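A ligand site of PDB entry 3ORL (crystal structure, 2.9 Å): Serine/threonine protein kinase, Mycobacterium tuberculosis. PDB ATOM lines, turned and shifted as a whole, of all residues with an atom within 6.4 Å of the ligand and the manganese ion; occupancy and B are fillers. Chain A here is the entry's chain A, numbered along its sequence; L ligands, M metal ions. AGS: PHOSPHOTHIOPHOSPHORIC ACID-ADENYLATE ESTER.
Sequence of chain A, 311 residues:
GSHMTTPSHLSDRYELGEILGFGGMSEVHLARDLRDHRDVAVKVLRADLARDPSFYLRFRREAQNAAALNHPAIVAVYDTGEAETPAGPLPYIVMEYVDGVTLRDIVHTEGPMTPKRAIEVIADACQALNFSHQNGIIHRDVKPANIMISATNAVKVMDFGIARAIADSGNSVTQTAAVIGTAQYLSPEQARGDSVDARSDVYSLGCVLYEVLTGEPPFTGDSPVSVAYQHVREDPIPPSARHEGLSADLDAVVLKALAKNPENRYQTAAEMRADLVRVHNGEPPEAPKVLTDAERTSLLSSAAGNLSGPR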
ATOM      1  N   LEU A  20     -36.404 -10.569 -20.824  1.00  0.00           N
ATOM      2  CA  LEU A  20     -35.493  -9.443 -20.613  1.00  0.00           C
ATOM      3  C   LEU A  20     -34.567  -9.280 -21.812  1.00  0.00           C
ATOM      4  O   LEU A  20     -34.143  -8.170 -22.132  1.00  0.00           O
ATOM      5  CB  LEU A  20     -34.697  -9.631 -19.315  1.00  0.00           C
ATOM      6  CG  LEU A  20     -35.465  -9.637 -17.975  1.00  0.00           C
ATOM      7  CD1 LEU A  20     -34.729 -10.459 -16.929  1.00  0.00           C
ATOM      8  CD2 LEU A  20     -35.727  -8.224 -17.467  1.00  0.00           C
ATOM      9  N   GLY A  21     -34.247 -10.407 -22.463  1.00  0.00           N
ATOM     10  CA  GLY A  21     -33.420 -10.393 -23.662  1.00  0.00           C
ATOM     11  C   GLY A  21     -32.959 -11.764 -24.111  1.00  0.00           C
ATOM     12  O   GLY A  21     -33.039 -12.751 -23.359  1.00  0.00           O
ATOM     13  N   PHE A  22     -32.472 -11.834 -25.348  1.00  0.00           N
ATOM     14  CA  PHE A  22     -31.952 -13.064 -25.952  1.00  0.00           C
ATOM     15  C   PHE A  22     -30.436 -13.018 -26.036  1.00  0.00           C
ATOM     16  O   PHE A  22     -29.853 -12.016 -26.463  1.00  0.00           O
ATOM     17  CB  PHE A  22     -32.523 -13.280 -27.352  1.00  0.00           C
ATOM     18  CG  PHE A  22     -34.004 -13.538 -27.381  1.00  0.00           C
ATOM     19  CD1 PHE A  22     -34.903 -12.473 -27.426  1.00  0.00           C
ATOM     20  CD2 PHE A  22     -34.497 -14.837 -27.357  1.00  0.00           C
ATOM     21  CE1 PHE A  22     -36.281 -12.695 -27.449  1.00  0.00           C
ATOM     22  CE2 PHE A  22     -35.866 -15.079 -27.374  1.00  0.00           C
ATOM     23  CZ  PHE A  22     -36.765 -14.005 -27.424  1.00  0.00           C
ATOM     24  N   GLY A  23     -29.813 -14.120 -25.613  1.00  0.00           N
ATOM     25  CA  GLY A  23     -28.383 -14.291 -25.799  1.00  0.00           C
ATOM     26  C   GLY A  23     -28.154 -15.302 -26.900  1.00  0.00           C
ATOM     27  O   GLY A  23     -29.112 -15.869 -27.444  1.00  0.00           O
ATOM     28  N   GLY A  24     -26.882 -15.540 -27.209  1.00  0.00           N
ATOM     29  CA  GLY A  24     -26.493 -16.428 -28.311  1.00  0.00           C
ATOM     30  C   GLY A  24     -27.173 -17.793 -28.329  1.00  0.00           C
ATOM     31  O   GLY A  24     -27.404 -18.353 -29.414  1.00  0.00           O
ATOM     32  N   MET A  25     -27.493 -18.322 -27.154  1.00  0.00           N
ATOM     33  CA  MET A  25     -28.167 -19.612 -27.060  1.00  0.00           C
ATOM     34  C   MET A  25     -29.127 -19.738 -25.859  1.00  0.00           C
ATOM     35  O   MET A  25     -29.181 -20.792 -25.204  1.00  0.00           O
ATOM     36  CB  MET A  25     -27.148 -20.767 -27.068  1.00  0.00           C
ATOM     37  CG  MET A  25     -26.174 -20.745 -25.881  1.00  0.00           C
ATOM     38  SD  MET A  25     -25.774 -22.434 -25.385  1.00  0.00           S
ATOM     39  CE  MET A  25     -24.472 -22.121 -24.162  1.00  0.00           C
ATOM     40  N   SER A  26     -29.891 -18.692 -25.587  1.00  0.00           N
ATOM     41  CA  SER A  26     -30.846 -18.694 -24.471  1.00  0.00           C
ATOM     42  C   SER A  26     -31.742 -17.463 -24.466  1.00  0.00           C
ATOM     43  O   SER A  26     -31.312 -16.346 -24.897  1.00  0.00           O
ATOM     44  CB  SER A  26     -30.085 -18.764 -23.125  1.00  0.00           C
ATOM     45  OG  SER A  26     -29.572 -17.478 -22.763  1.00  0.00           O
ATOM     46  N   GLU A  27     -32.973 -17.673 -23.974  1.00  0.00           N
ATOM     47  CA  GLU A  27     -33.844 -16.536 -23.645  1.00  0.00           C
ATOM     48  C   GLU A  27     -33.836 -16.343 -22.137  1.00  0.00           C
ATOM     49  O   GLU A  27     -34.044 -17.304 -21.383  1.00  0.00           O
ATOM     50  CB  GLU A  27     -35.260 -16.723 -24.199  1.00  0.00           C
ATOM     51  CG  GLU A  27     -35.956 -18.039 -23.802  1.00  0.00           C
ATOM     52  CD  GLU A  27     -37.378 -18.141 -24.347  1.00  0.00           C
ATOM     53  OE1 GLU A  27     -37.812 -17.246 -25.114  1.00  0.00           O
ATOM     54  OE2 GLU A  27     -38.075 -19.129 -24.000  1.00  0.00           O
ATOM     55  N   VAL A  28     -33.577 -15.115 -21.699  1.00  0.00           N
ATOM     56  CA  VAL A  28     -33.540 -14.807 -20.272  1.00  0.00           C
ATOM     57  C   VAL A  28     -34.829 -14.102 -19.845  1.00  0.00           C
ATOM     58  O   VAL A  28     -35.135 -12.999 -20.299  1.00  0.00           O
ATOM     59  CB  VAL A  28     -32.297 -13.960 -19.895  1.00  0.00           C
ATOM     60  CG1 VAL A  28     -32.132 -13.914 -18.379  1.00  0.00           C
ATOM     61  CG2 VAL A  28     -31.042 -14.527 -20.547  1.00  0.00           C
ATOM     62  N   HIS A  29     -35.589 -14.774 -18.979  1.00  0.00           N
ATOM     63  CA  HIS A  29     -36.864 -14.259 -18.481  1.00  0.00           C
ATOM     64  C   HIS A  29     -36.725 -13.608 -17.114  1.00  0.00           C
ATOM     65  O   HIS A  29     -35.806 -13.924 -16.345  1.00  0.00           O
ATOM     66  CB  HIS A  29     -37.886 -15.388 -18.373  1.00  0.00           C
ATOM     67  CG  HIS A  29     -38.460 -15.824 -19.676  1.00  0.00           C
ATOM     68  ND1 HIS A  29     -39.696 -15.393 -20.123  1.00  0.00           N
ATOM     69  CD2 HIS A  29     -37.975 -16.656 -20.634  1.00  0.00           C
ATOM     70  CE1 HIS A  29     -39.948 -15.948 -21.303  1.00  0.00           C
ATOM     71  NE2 HIS A  29     -38.913 -16.717 -21.626  1.00  0.00           N
ATOM     72  N   ALA A  41     -34.061 -13.730 -11.993  1.00  0.00           N
ATOM     73  CA  ALA A  41     -33.843 -13.878 -13.435  1.00  0.00           C
ATOM     74  C   ALA A  41     -33.582 -15.343 -13.771  1.00  0.00           C
ATOM     75  O   ALA A  41     -32.843 -16.033 -13.061  1.00  0.00           O
ATOM     76  CB  ALA A  41     -32.688 -13.010 -13.902  1.00  0.00           C
ATOM     77  N   LYS A  43     -32.396 -17.909 -16.881  1.00  0.00           N
ATOM     78  CA  LYS A  43     -31.831 -18.122 -18.206  1.00  0.00           C
ATOM     79  C   LYS A  43     -32.196 -19.517 -18.719  1.00  0.00           C
ATOM     80  O   LYS A  43     -31.688 -20.523 -18.211  1.00  0.00           O
ATOM     81  CB  LYS A  43     -30.315 -17.901 -18.204  1.00  0.00           C
ATOM     82  CG  LYS A  43     -29.674 -17.916 -19.582  1.00  0.00           C
ATOM     83  CD  LYS A  43     -28.155 -17.831 -19.494  1.00  0.00           C
ATOM     84  CE  LYS A  43     -27.695 -16.423 -19.100  1.00  0.00           C
ATOM     85  NZ  LYS A  43     -26.200 -16.331 -19.040  1.00  0.00           N
ATOM     86  N   PHE A  59     -25.296 -26.027 -22.907  1.00  0.00           N
ATOM     87  CA  PHE A  59     -26.015 -25.290 -21.878  1.00  0.00           C
ATOM     88  C   PHE A  59     -25.948 -26.047 -20.549  1.00  0.00           C
ATOM     89  O   PHE A  59     -25.580 -25.465 -19.523  1.00  0.00           O
ATOM     90  CB  PHE A  59     -27.476 -25.065 -22.291  1.00  0.00           C
ATOM     91  CG  PHE A  59     -28.214 -24.060 -21.438  1.00  0.00           C
ATOM     92  CD1 PHE A  59     -28.364 -22.746 -21.860  1.00  0.00           C
ATOM     93  CD2 PHE A  59     -28.760 -24.437 -20.204  1.00  0.00           C
ATOM     94  CE1 PHE A  59     -29.053 -21.814 -21.076  1.00  0.00           C
ATOM     95  CE2 PHE A  59     -29.449 -23.514 -19.415  1.00  0.00           C
ATOM     96  CZ  PHE A  59     -29.595 -22.198 -19.853  1.00  0.00           C
ATOM     97  N   GLU A  62     -22.475 -25.497 -18.990  1.00  0.00           N
ATOM     98  CA  GLU A  62     -22.331 -24.115 -18.526  1.00  0.00           C
ATOM     99  C   GLU A  62     -23.360 -23.704 -17.474  1.00  0.00           C
ATOM    100  O   GLU A  62     -23.340 -22.560 -17.008  1.00  0.00           O
ATOM    101  CB  GLU A  62     -22.409 -23.143 -19.718  1.00  0.00           C
ATOM    102  CG  GLU A  62     -21.287 -23.292 -20.752  1.00  0.00           C
ATOM    103  CD  GLU A  62     -21.194 -22.103 -21.716  1.00  0.00           C
ATOM    104  OE1 GLU A  62     -22.077 -21.197 -21.657  1.00  0.00           O
ATOM    105  OE2 GLU A  62     -20.229 -22.063 -22.520  1.00  0.00           O
ATOM    106  N   VAL A  75     -22.945 -11.450 -10.016  1.00  0.00           N
ATOM    107  CA  VAL A  75     -24.313 -11.957 -10.137  1.00  0.00           C
ATOM    108  C   VAL A  75     -24.411 -13.310  -9.445  1.00  0.00           C
ATOM    109  O   VAL A  75     -23.746 -14.271  -9.832  1.00  0.00           O
ATOM    110  CB  VAL A  75     -24.740 -12.086 -11.624  1.00  0.00           C
ATOM    111  CG1 VAL A  75     -26.137 -12.696 -11.746  1.00  0.00           C
ATOM    112  CG2 VAL A  75     -24.704 -10.726 -12.306  1.00  0.00           C
ATOM    113  N   MET A  95     -30.855 -16.910 -11.302  1.00  0.00           N
ATOM    114  CA  MET A  95     -29.830 -16.007 -10.791  1.00  0.00           C
ATOM    115  C   MET A  95     -30.369 -14.644 -10.380  1.00  0.00           C
ATOM    116  O   MET A  95     -31.539 -14.343 -10.588  1.00  0.00           O
ATOM    117  CB  MET A  95     -28.706 -15.842 -11.817  1.00  0.00           C
ATOM    118  CG  MET A  95     -29.219 -15.723 -13.295  1.00  0.00           C
ATOM    119  SD  MET A  95     -27.840 -15.095 -14.346  1.00  0.00           S
ATOM    120  CE  MET A  95     -26.442 -16.189 -13.910  1.00  0.00           C
ATOM    121  N   GLU A  96     -29.487 -13.837  -9.777  1.00  0.00           N
ATOM    122  CA  GLU A  96     -29.820 -12.491  -9.330  1.00  0.00           C
ATOM    123  C   GLU A  96     -30.343 -11.636 -10.476  1.00  0.00           C
ATOM    124  O   GLU A  96     -29.716 -11.543 -11.540  1.00  0.00           O
ATOM    125  CB  GLU A  96     -28.610 -11.823  -8.702  1.00  0.00           C
ATOM    126  CG  GLU A  96     -28.911 -10.487  -8.086  1.00  0.00           C
ATOM    127  CD  GLU A  96     -27.668  -9.681  -7.804  1.00  0.00           C
ATOM    128  OE1 GLU A  96     -26.694 -10.255  -7.268  1.00  0.00           O
ATOM    129  OE2 GLU A  96     -27.665  -8.457  -8.116  1.00  0.00           O
ATOM    130  N   TYR A  97     -31.513 -11.031 -10.265  1.00  0.00           N
ATOM    131  CA  TYR A  97     -32.108 -10.169 -11.279  1.00  0.00           C
ATOM    132  C   TYR A  97     -31.369  -8.835 -11.334  1.00  0.00           C
ATOM    133  O   TYR A  97     -31.390  -8.057 -10.379  1.00  0.00           O
ATOM    134  CB  TYR A  97     -33.596  -9.957 -11.001  1.00  0.00           C
ATOM    135  CG  TYR A  97     -34.209  -8.846 -11.815  1.00  0.00           C
ATOM    136  CD1 TYR A  97     -34.232  -8.918 -13.210  1.00  0.00           C
ATOM    137  CD2 TYR A  97     -34.754  -7.725 -11.200  1.00  0.00           C
ATOM    138  CE1 TYR A  97     -34.796  -7.890 -13.969  1.00  0.00           C
ATOM    139  CE2 TYR A  97     -35.321  -6.691 -11.947  1.00  0.00           C
ATOM    140  CZ  TYR A  97     -35.337  -6.791 -13.332  1.00  0.00           C
ATOM    141  OH  TYR A  97     -35.887  -5.780 -14.077  1.00  0.00           O
ATOM    142  N   VAL A  98     -30.729  -8.576 -12.471  1.00  0.00           N
ATOM    143  CA  VAL A  98     -30.055  -7.303 -12.699  1.00  0.00           C
ATOM    144  C   VAL A  98     -30.938  -6.441 -13.596  1.00  0.00           C
ATOM    145  O   VAL A  98     -31.082  -6.718 -14.788  1.00  0.00           O
ATOM    146  CB  VAL A  98     -28.640  -7.504 -13.328  1.00  0.00           C
ATOM    147  CG1 VAL A  98     -27.874  -6.175 -13.372  1.00  0.00           C
ATOM    148  CG2 VAL A  98     -27.848  -8.552 -12.559  1.00  0.00           C
ATOM    149  N   ASP A  99     -31.540  -5.403 -13.029  1.00  0.00           N
ATOM    150  CA  ASP A  99     -32.314  -4.450 -13.823  1.00  0.00           C
ATOM    151  C   ASP A  99     -31.359  -3.538 -14.566  1.00  0.00           C
ATOM    152  O   ASP A  99     -30.898  -2.532 -14.029  1.00  0.00           O
ATOM    153  CB  ASP A  99     -33.286  -3.651 -12.956  1.00  0.00           C
ATOM    154  CG  ASP A  99     -33.996  -2.531 -13.738  1.00  0.00           C
ATOM    155  OD1 ASP A  99     -34.178  -2.670 -14.971  1.00  0.00           O
ATOM    156  OD2 ASP A  99     -34.360  -1.521 -13.112  1.00  0.00           O
ATOM    157  N   GLY A 100     -31.047  -3.896 -15.808  1.00  0.00           N
ATOM    158  CA  GLY A 100     -30.143  -3.110 -16.632  1.00  0.00           C
ATOM    159  C   GLY A 100     -29.754  -3.856 -17.890  1.00  0.00           C
ATOM    160  O   GLY A 100     -30.508  -4.700 -18.370  1.00  0.00           O
ATOM    161  N   VAL A 101     -28.574  -3.543 -18.406  1.00  0.00           N
ATOM    162  CA  VAL A 101     -28.081  -4.129 -19.661  1.00  0.00           C
ATOM    163  C   VAL A 101     -26.643  -4.631 -19.538  1.00  0.00           C
ATOM    164  O   VAL A 101     -25.931  -4.272 -18.594  1.00  0.00           O
ATOM    165  CB  VAL A 101     -28.203  -3.128 -20.843  1.00  0.00           C
ATOM    166  CG1 VAL A 101     -29.661  -2.643 -20.997  1.00  0.00           C
ATOM    167  CG2 VAL A 101     -27.264  -1.945 -20.654  1.00  0.00           C
ATOM    168  N   THR A 102     -26.216  -5.463 -20.499  1.00  0.00           N
ATOM    169  CA  THR A 102     -24.827  -5.907 -20.559  1.00  0.00           C
ATOM    170  C   THR A 102     -24.043  -4.929 -21.413  1.00  0.00           C
ATOM    171  O   THR A 102     -24.632  -4.200 -22.213  1.00  0.00           O
ATOM    172  CB  THR A 102     -24.654  -7.315 -21.184  1.00  0.00           C
ATOM    173  OG1 THR A 102     -24.749  -7.221 -22.613  1.00  0.00           O
ATOM    174  CG2 THR A 102     -25.685  -8.299 -20.654  1.00  0.00           C
ATOM    175  N   ARG A 104     -22.383  -5.529 -23.950  1.00  0.00           N
ATOM    176  CA  ARG A 104     -22.664  -5.809 -25.355  1.00  0.00           C
ATOM    177  C   ARG A 104     -23.820  -4.935 -25.850  1.00  0.00           C
ATOM    178  O   ARG A 104     -23.672  -4.223 -26.846  1.00  0.00           O
ATOM    179  CB  ARG A 104     -22.970  -7.293 -25.596  1.00  0.00           C
ATOM    180  CG  ARG A 104     -23.245  -7.625 -27.053  1.00  0.00           C
ATOM    181  CD  ARG A 104     -23.354  -9.118 -27.284  1.00  0.00           C
ATOM    182  NE  ARG A 104     -24.483  -9.709 -26.568  1.00  0.00           N
ATOM    183  CZ  ARG A 104     -24.761 -11.013 -26.547  1.00  0.00           C
ATOM    184  NH1 ARG A 104     -23.995 -11.877 -27.209  1.00  0.00           N
ATOM    185  NH2 ARG A 104     -25.819 -11.445 -25.873  1.00  0.00           N
ATOM    186  N   ASP A 105     -24.959  -4.988 -25.137  1.00  0.00           N
ATOM    187  CA  ASP A 105     -26.133  -4.170 -25.446  1.00  0.00           C
ATOM    188  C   ASP A 105     -25.753  -2.711 -25.657  1.00  0.00           C
ATOM    189  O   ASP A 105     -26.159  -2.104 -26.649  1.00  0.00           O
ATOM    190  CB  ASP A 105     -27.194  -4.283 -24.345  1.00  0.00           C
ATOM    191  CG  ASP A 105     -27.487  -5.724 -23.938  1.00  0.00           C
ATOM    192  OD1 ASP A 105     -27.360  -6.645 -24.778  1.00  0.00           O
ATOM    193  OD2 ASP A 105     -27.851  -5.937 -22.754  1.00  0.00           O
ATOM    194  N   ASP A 141     -13.842 -16.393 -19.183  1.00  0.00           N
ATOM    195  CA  ASP A 141     -14.889 -16.128 -20.167  1.00  0.00           C
ATOM    196  C   ASP A 141     -15.346 -14.668 -20.071  1.00  0.00           C
ATOM    197  O   ASP A 141     -16.534 -14.366 -20.176  1.00  0.00           O
ATOM    198  CB  ASP A 141     -16.064 -17.099 -19.945  1.00  0.00           C
ATOM    199  CG  ASP A 141     -17.028 -17.121 -21.112  1.00  0.00           C
ATOM    200  OD1 ASP A 141     -16.680 -16.647 -22.221  1.00  0.00           O
ATOM    201  OD2 ASP A 141     -18.153 -17.635 -20.912  1.00  0.00           O
ATOM    202  N   LYS A 143     -16.164 -11.127 -21.220  1.00  0.00           N
ATOM    203  CA  LYS A 143     -16.648 -10.516 -22.452  1.00  0.00           C
ATOM    204  C   LYS A 143     -17.775  -9.530 -22.113  1.00  0.00           C
ATOM    205  O   LYS A 143     -18.300  -9.559 -20.994  1.00  0.00           O
ATOM    206  CB  LYS A 143     -17.108 -11.586 -23.451  1.00  0.00           C
ATOM    207  CG  LYS A 143     -18.064 -12.636 -22.893  1.00  0.00           C
ATOM    208  CD  LYS A 143     -18.216 -13.781 -23.875  1.00  0.00           C
ATOM    209  CE  LYS A 143     -19.388 -14.677 -23.500  1.00  0.00           C
ATOM    210  NZ  LYS A 143     -20.676 -13.945 -23.637  1.00  0.00           N
ATOM    211  N   ALA A 145     -20.923  -9.326 -22.935  1.00  0.00           N
ATOM    212  CA  ALA A 145     -22.221  -9.920 -22.595  1.00  0.00           C
ATOM    213  C   ALA A 145     -22.258 -10.509 -21.174  1.00  0.00           C
ATOM    214  O   ALA A 145     -23.326 -10.835 -20.657  1.00  0.00           O
ATOM    215  CB  ALA A 145     -22.626 -10.968 -23.614  1.00  0.00           C
ATOM    216  N   ASN A 146     -21.078 -10.633 -20.547  1.00  0.00           N
ATOM    217  CA  ASN A 146     -20.967 -11.167 -19.186  1.00  0.00           C
ATOM    218  C   ASN A 146     -20.708 -10.103 -18.122  1.00  0.00           C
ATOM    219  O   ASN A 146     -20.454 -10.432 -16.965  1.00  0.00           O
ATOM    220  CB  ASN A 146     -19.871 -12.238 -19.106  1.00  0.00           C
ATOM    221  CG  ASN A 146     -20.325 -13.587 -19.641  1.00  0.00           C
ATOM    222  OD1 ASN A 146     -21.508 -13.943 -19.610  1.00  0.00           O
ATOM    223  ND2 ASN A 146     -19.363 -14.379 -20.127  1.00  0.00           N
ATOM    224  N   MET A 148     -22.531  -6.610 -16.584  1.00  0.00           N
ATOM    225  CA  MET A 148     -23.777  -5.834 -16.562  1.00  0.00           C
ATOM    226  C   MET A 148     -23.706  -4.514 -15.781  1.00  0.00           C
ATOM    227  O   MET A 148     -22.858  -4.332 -14.904  1.00  0.00           O
ATOM    228  CB  MET A 148     -24.929  -6.687 -16.027  1.00  0.00           C
ATOM    229  CG  MET A 148     -25.383  -7.777 -16.979  1.00  0.00           C
ATOM    230  SD  MET A 148     -27.017  -8.430 -16.589  1.00  0.00           S
ATOM    231  CE  MET A 148     -28.075  -7.041 -17.064  1.00  0.00           C
ATOM    232  N   MET A 158     -21.020 -11.808 -14.344  1.00  0.00           N
ATOM    233  CA  MET A 158     -21.677 -13.123 -14.272  1.00  0.00           C
ATOM    234  C   MET A 158     -20.991 -14.203 -15.117  1.00  0.00           C
ATOM    235  O   MET A 158     -20.194 -13.888 -16.005  1.00  0.00           O
ATOM    236  CB  MET A 158     -23.133 -13.012 -14.704  1.00  0.00           C
ATOM    237  CG  MET A 158     -23.296 -12.597 -16.176  1.00  0.00           C
ATOM    238  SD  MET A 158     -25.013 -12.192 -16.539  1.00  0.00           S
ATOM    239  CE  MET A 158     -24.824 -11.223 -18.056  1.00  0.00           C
ATOM    240  N   ASP A 159     -21.340 -15.456 -14.844  1.00  0.00           N
ATOM    241  CA  ASP A 159     -20.818 -16.638 -15.567  1.00  0.00           C
ATOM    242  C   ASP A 159     -19.370 -16.995 -15.268  1.00  0.00           C
ATOM    243  O   ASP A 159     -18.624 -17.425 -16.157  1.00  0.00           O
ATOM    244  CB  ASP A 159     -21.036 -16.501 -17.085  1.00  0.00           C
ATOM    245  CG  ASP A 159     -22.500 -16.535 -17.471  1.00  0.00           C
ATOM    246  OD1 ASP A 159     -23.381 -16.567 -16.568  1.00  0.00           O
ATOM    247  OD2 ASP A 159     -22.770 -16.518 -18.693  1.00  0.00           O
ATOM    248  N   ILE A 162     -16.666 -22.179 -15.974  1.00  0.00           N
ATOM    249  CA  ILE A 162     -16.921 -22.660 -17.349  1.00  0.00           C
ATOM    250  C   ILE A 162     -15.602 -22.979 -18.088  1.00  0.00           C
ATOM    251  O   ILE A 162     -15.076 -22.141 -18.870  1.00  0.00           O
ATOM    252  CB  ILE A 162     -17.798 -21.673 -18.188  1.00  0.00           C
ATOM    253  CG1 ILE A 162     -19.116 -21.346 -17.455  1.00  0.00           C
ATOM    254  CG2 ILE A 162     -18.074 -22.235 -19.584  1.00  0.00           C
ATOM    255  CD1 ILE A 162     -19.827 -20.069 -17.997  1.00  0.00           C
ATOM    256  N   THR A 182     -17.379 -14.700 -28.066  1.00  0.00           N
ATOM    257  CA  THR A 182     -16.174 -15.001 -27.305  1.00  0.00           C
ATOM    258  C   THR A 182     -14.968 -15.319 -28.207  1.00  0.00           C
ATOM    259  O   THR A 182     -13.905 -15.730 -27.727  1.00  0.00           O
ATOM    260  CB  THR A 182     -16.415 -16.149 -26.270  1.00  0.00           C
ATOM    261  OG1 THR A 182     -15.372 -16.139 -25.265  1.00  0.00           O
ATOM    262  CG2 THR A 182     -16.490 -17.536 -26.945  1.00  0.00           C
HETATM  263  PG  AGS L   1     -23.920 -15.485 -24.441  1.00  0.00           P
HETATM  264  S1G AGS L   1     -23.785 -17.167 -24.839  1.00  0.00           S
HETATM  265  O2G AGS L   1     -23.160 -14.500 -25.466  1.00  0.00           O
HETATM  266  O3G AGS L   1     -23.295 -15.259 -23.002  1.00  0.00           O
HETATM  267  PB  AGS L   1     -26.483 -15.931 -23.340  1.00  0.00           P
HETATM  268  O1B AGS L   1     -27.264 -16.956 -24.082  1.00  0.00           O
HETATM  269  O2B AGS L   1     -25.707 -16.591 -22.188  1.00  0.00           O
HETATM  270  O3B AGS L   1     -25.515 -15.163 -24.378  1.00  0.00           O
HETATM  271  PA  AGS L   1     -26.886 -13.449 -22.013  1.00  0.00           P
HETATM  272  O1A AGS L   1     -26.157 -13.862 -20.770  1.00  0.00           O
HETATM  273  O2A AGS L   1     -26.008 -12.546 -22.937  1.00  0.00           O
HETATM  274  O3A AGS L   1     -27.448 -14.762 -22.773  1.00  0.00           O
HETATM  275  O5' AGS L   1     -28.218 -12.628 -21.648  1.00  0.00           O
HETATM  276  C5' AGS L   1     -28.974 -12.117 -22.718  1.00  0.00           C
HETATM  277  C4' AGS L   1     -29.812 -10.937 -22.251  1.00  0.00           C
HETATM  278  O4' AGS L   1     -30.564 -11.328 -21.128  1.00  0.00           O
HETATM  279  C3' AGS L   1     -28.973  -9.753 -21.817  1.00  0.00           C
HETATM  280  O3' AGS L   1     -28.776  -8.838 -22.878  1.00  0.00           O
HETATM  281  C2' AGS L   1     -29.764  -9.162 -20.662  1.00  0.00           C
HETATM  282  O2' AGS L   1     -30.692  -8.191 -21.120  1.00  0.00           O
HETATM  283  C1' AGS L   1     -30.568 -10.337 -20.118  1.00  0.00           C
HETATM  284  N9  AGS L   1     -29.938 -10.872 -18.889  1.00  0.00           N
HETATM  285  C8  AGS L   1     -28.904 -11.778 -18.822  1.00  0.00           C
HETATM  286  N7  AGS L   1     -28.616 -12.018 -17.527  1.00  0.00           N
HETATM  287  C5  AGS L   1     -29.450 -11.289 -16.760  1.00  0.00           C
HETATM  288  C6  AGS L   1     -29.591 -11.157 -15.385  1.00  0.00           C
HETATM  289  N6  AGS L   1     -28.818 -11.877 -14.563  1.00  0.00           N
HETATM  290  N1  AGS L   1     -30.560 -10.315 -14.870  1.00  0.00           N
HETATM  291  C2  AGS L   1     -31.388  -9.614 -15.726  1.00  0.00           C
HETATM  292  N3  AGS L   1     -31.242  -9.733 -17.098  1.00  0.00           N
HETATM  293  C4  AGS L   1     -30.291 -10.561 -17.609  1.00  0.00           C
HETATM  294 MN    MN M   1     -23.513 -16.599 -21.614  1.00  0.00          MN
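The side-chain sulfur of Met 158 sits close to a nitrogen (N7) of the ligand (3.7 Å). CD1 of Leu 20 touches N3 of the ligand, at 3.6 Å. O of Gly 21 touches O4' of the ligand, 3.6 Å away. Phe 22 touches the ligand. CA of Gly 23 touches O3A of the ligand (3.2 Å). Val 28 touches the ligand (CG2 to O4', 3.3 Å). Ala 41 touches the ligand. Val 75 touches the ligand. Tyr 97 touches the ligand (CD1 to C2, 3.9 Å). Thr 102 touches the ligand (CG2 to C3', 3.8 Å). CB of Ala 145 touches O2A of the ligand, at 3.8 Å. Met 148 touches the ligand (SD to C5, 3.8 Å). Hydrophobic or aromatic side chains that line the ligand: Leu 20, Val 28, Ala 41, Val 75, Met 95, Tyr 97, Val 98, Ala 145, Met 148 and Met 158.
The backbone NH of Ser 26 lies close to an oxygen (O1B) of the ligand, 3.5 Å away. The side-chain hydroxyl (OG) of Ser 26 lies within hydrogen-bond range of an oxygen (O1B) of the ligand (2.7 Å). N1 of the ligand is in hydrogen-bond range of N of Val 98 (3.0 Å). An oxygen (O2G) of the ligand is in hydrogen-bond range of the side-chain amino group (NZ) of Lys 143, 3.1 Å away. NZ of Lys 43 lies within salt-bridge range of O1A of the ligand (3.0 Å). An oxygen (O3') of the ligand is in hydrogen-bond range of the side-chain carboxylate (OD2) of Asp 105 (3.0 Å). NH2 of Arg 104 is in salt-bridge range of O2A of the ligand, at 3.1 Å. An oxygen (O3B) of the ligand lies within hydrogen-bond range of the backbone NH of Gly 24 (3.2 Å). N6 of the ligand lies within hydrogen-bond range of O of Glu 96. An oxygen (O1B) of the ligand is in hydrogen-bond range of the backbone NH (N) of Met 25 (3.4 Å). The side-chain sulfur of Met 95 lies within hydrogen-bond range of a nitrogen (N6) of the ligand (3.4 Å).
Residues that only touch the manganese ion: Lys 43 (3.7 Å), Asn 146 (3.9 Å) and Asp 159 (3.0 Å). Of the 34 residues printed, 3 come within 4 Å of the manganese ion.
The manganese ion is bound by an oxygen (O3G) of the ligand (1.9 Å) and an oxygen (O2B) of the ligand (2.3 Å). The manganese ion has two donor atoms within binding distance.
OD2 of Asp 159 lies within salt-bridge range of NZ of Lys 43, at 3.5 Å. OD1 of Asn 146 sits close to OD2 of Asp 159 (3.0 Å). The side-chain hydroxyl (OG1) of Thr 102 sits close to the backbone NH (N) of Arg 104 (3.2 Å). The backbone carbonyl oxygen (O) of Val 28 sits at hydrogen-bond distance from the backbone NH (N) of Leu 20. The backbone carbonyl oxygen (O) of Gly 21 sits at hydrogen-bond distance from the backbone NH (N) of Val 28, at 2.9 Å. The backbone NH (N) of Met 95 sits at hydrogen-bond distance from the backbone carbonyl oxygen (O) of Ala 41. The backbone NH (N) of Met 158 sits at hydrogen-bond distance from the backbone carbonyl oxygen (O) of Asn 146, at 3.0 Å. The side-chain amide nitrogen (ND2) of Asn 146 is in hydrogen-bond range of the backbone carbonyl oxygen (O) of Asp 141 (2.8 Å).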
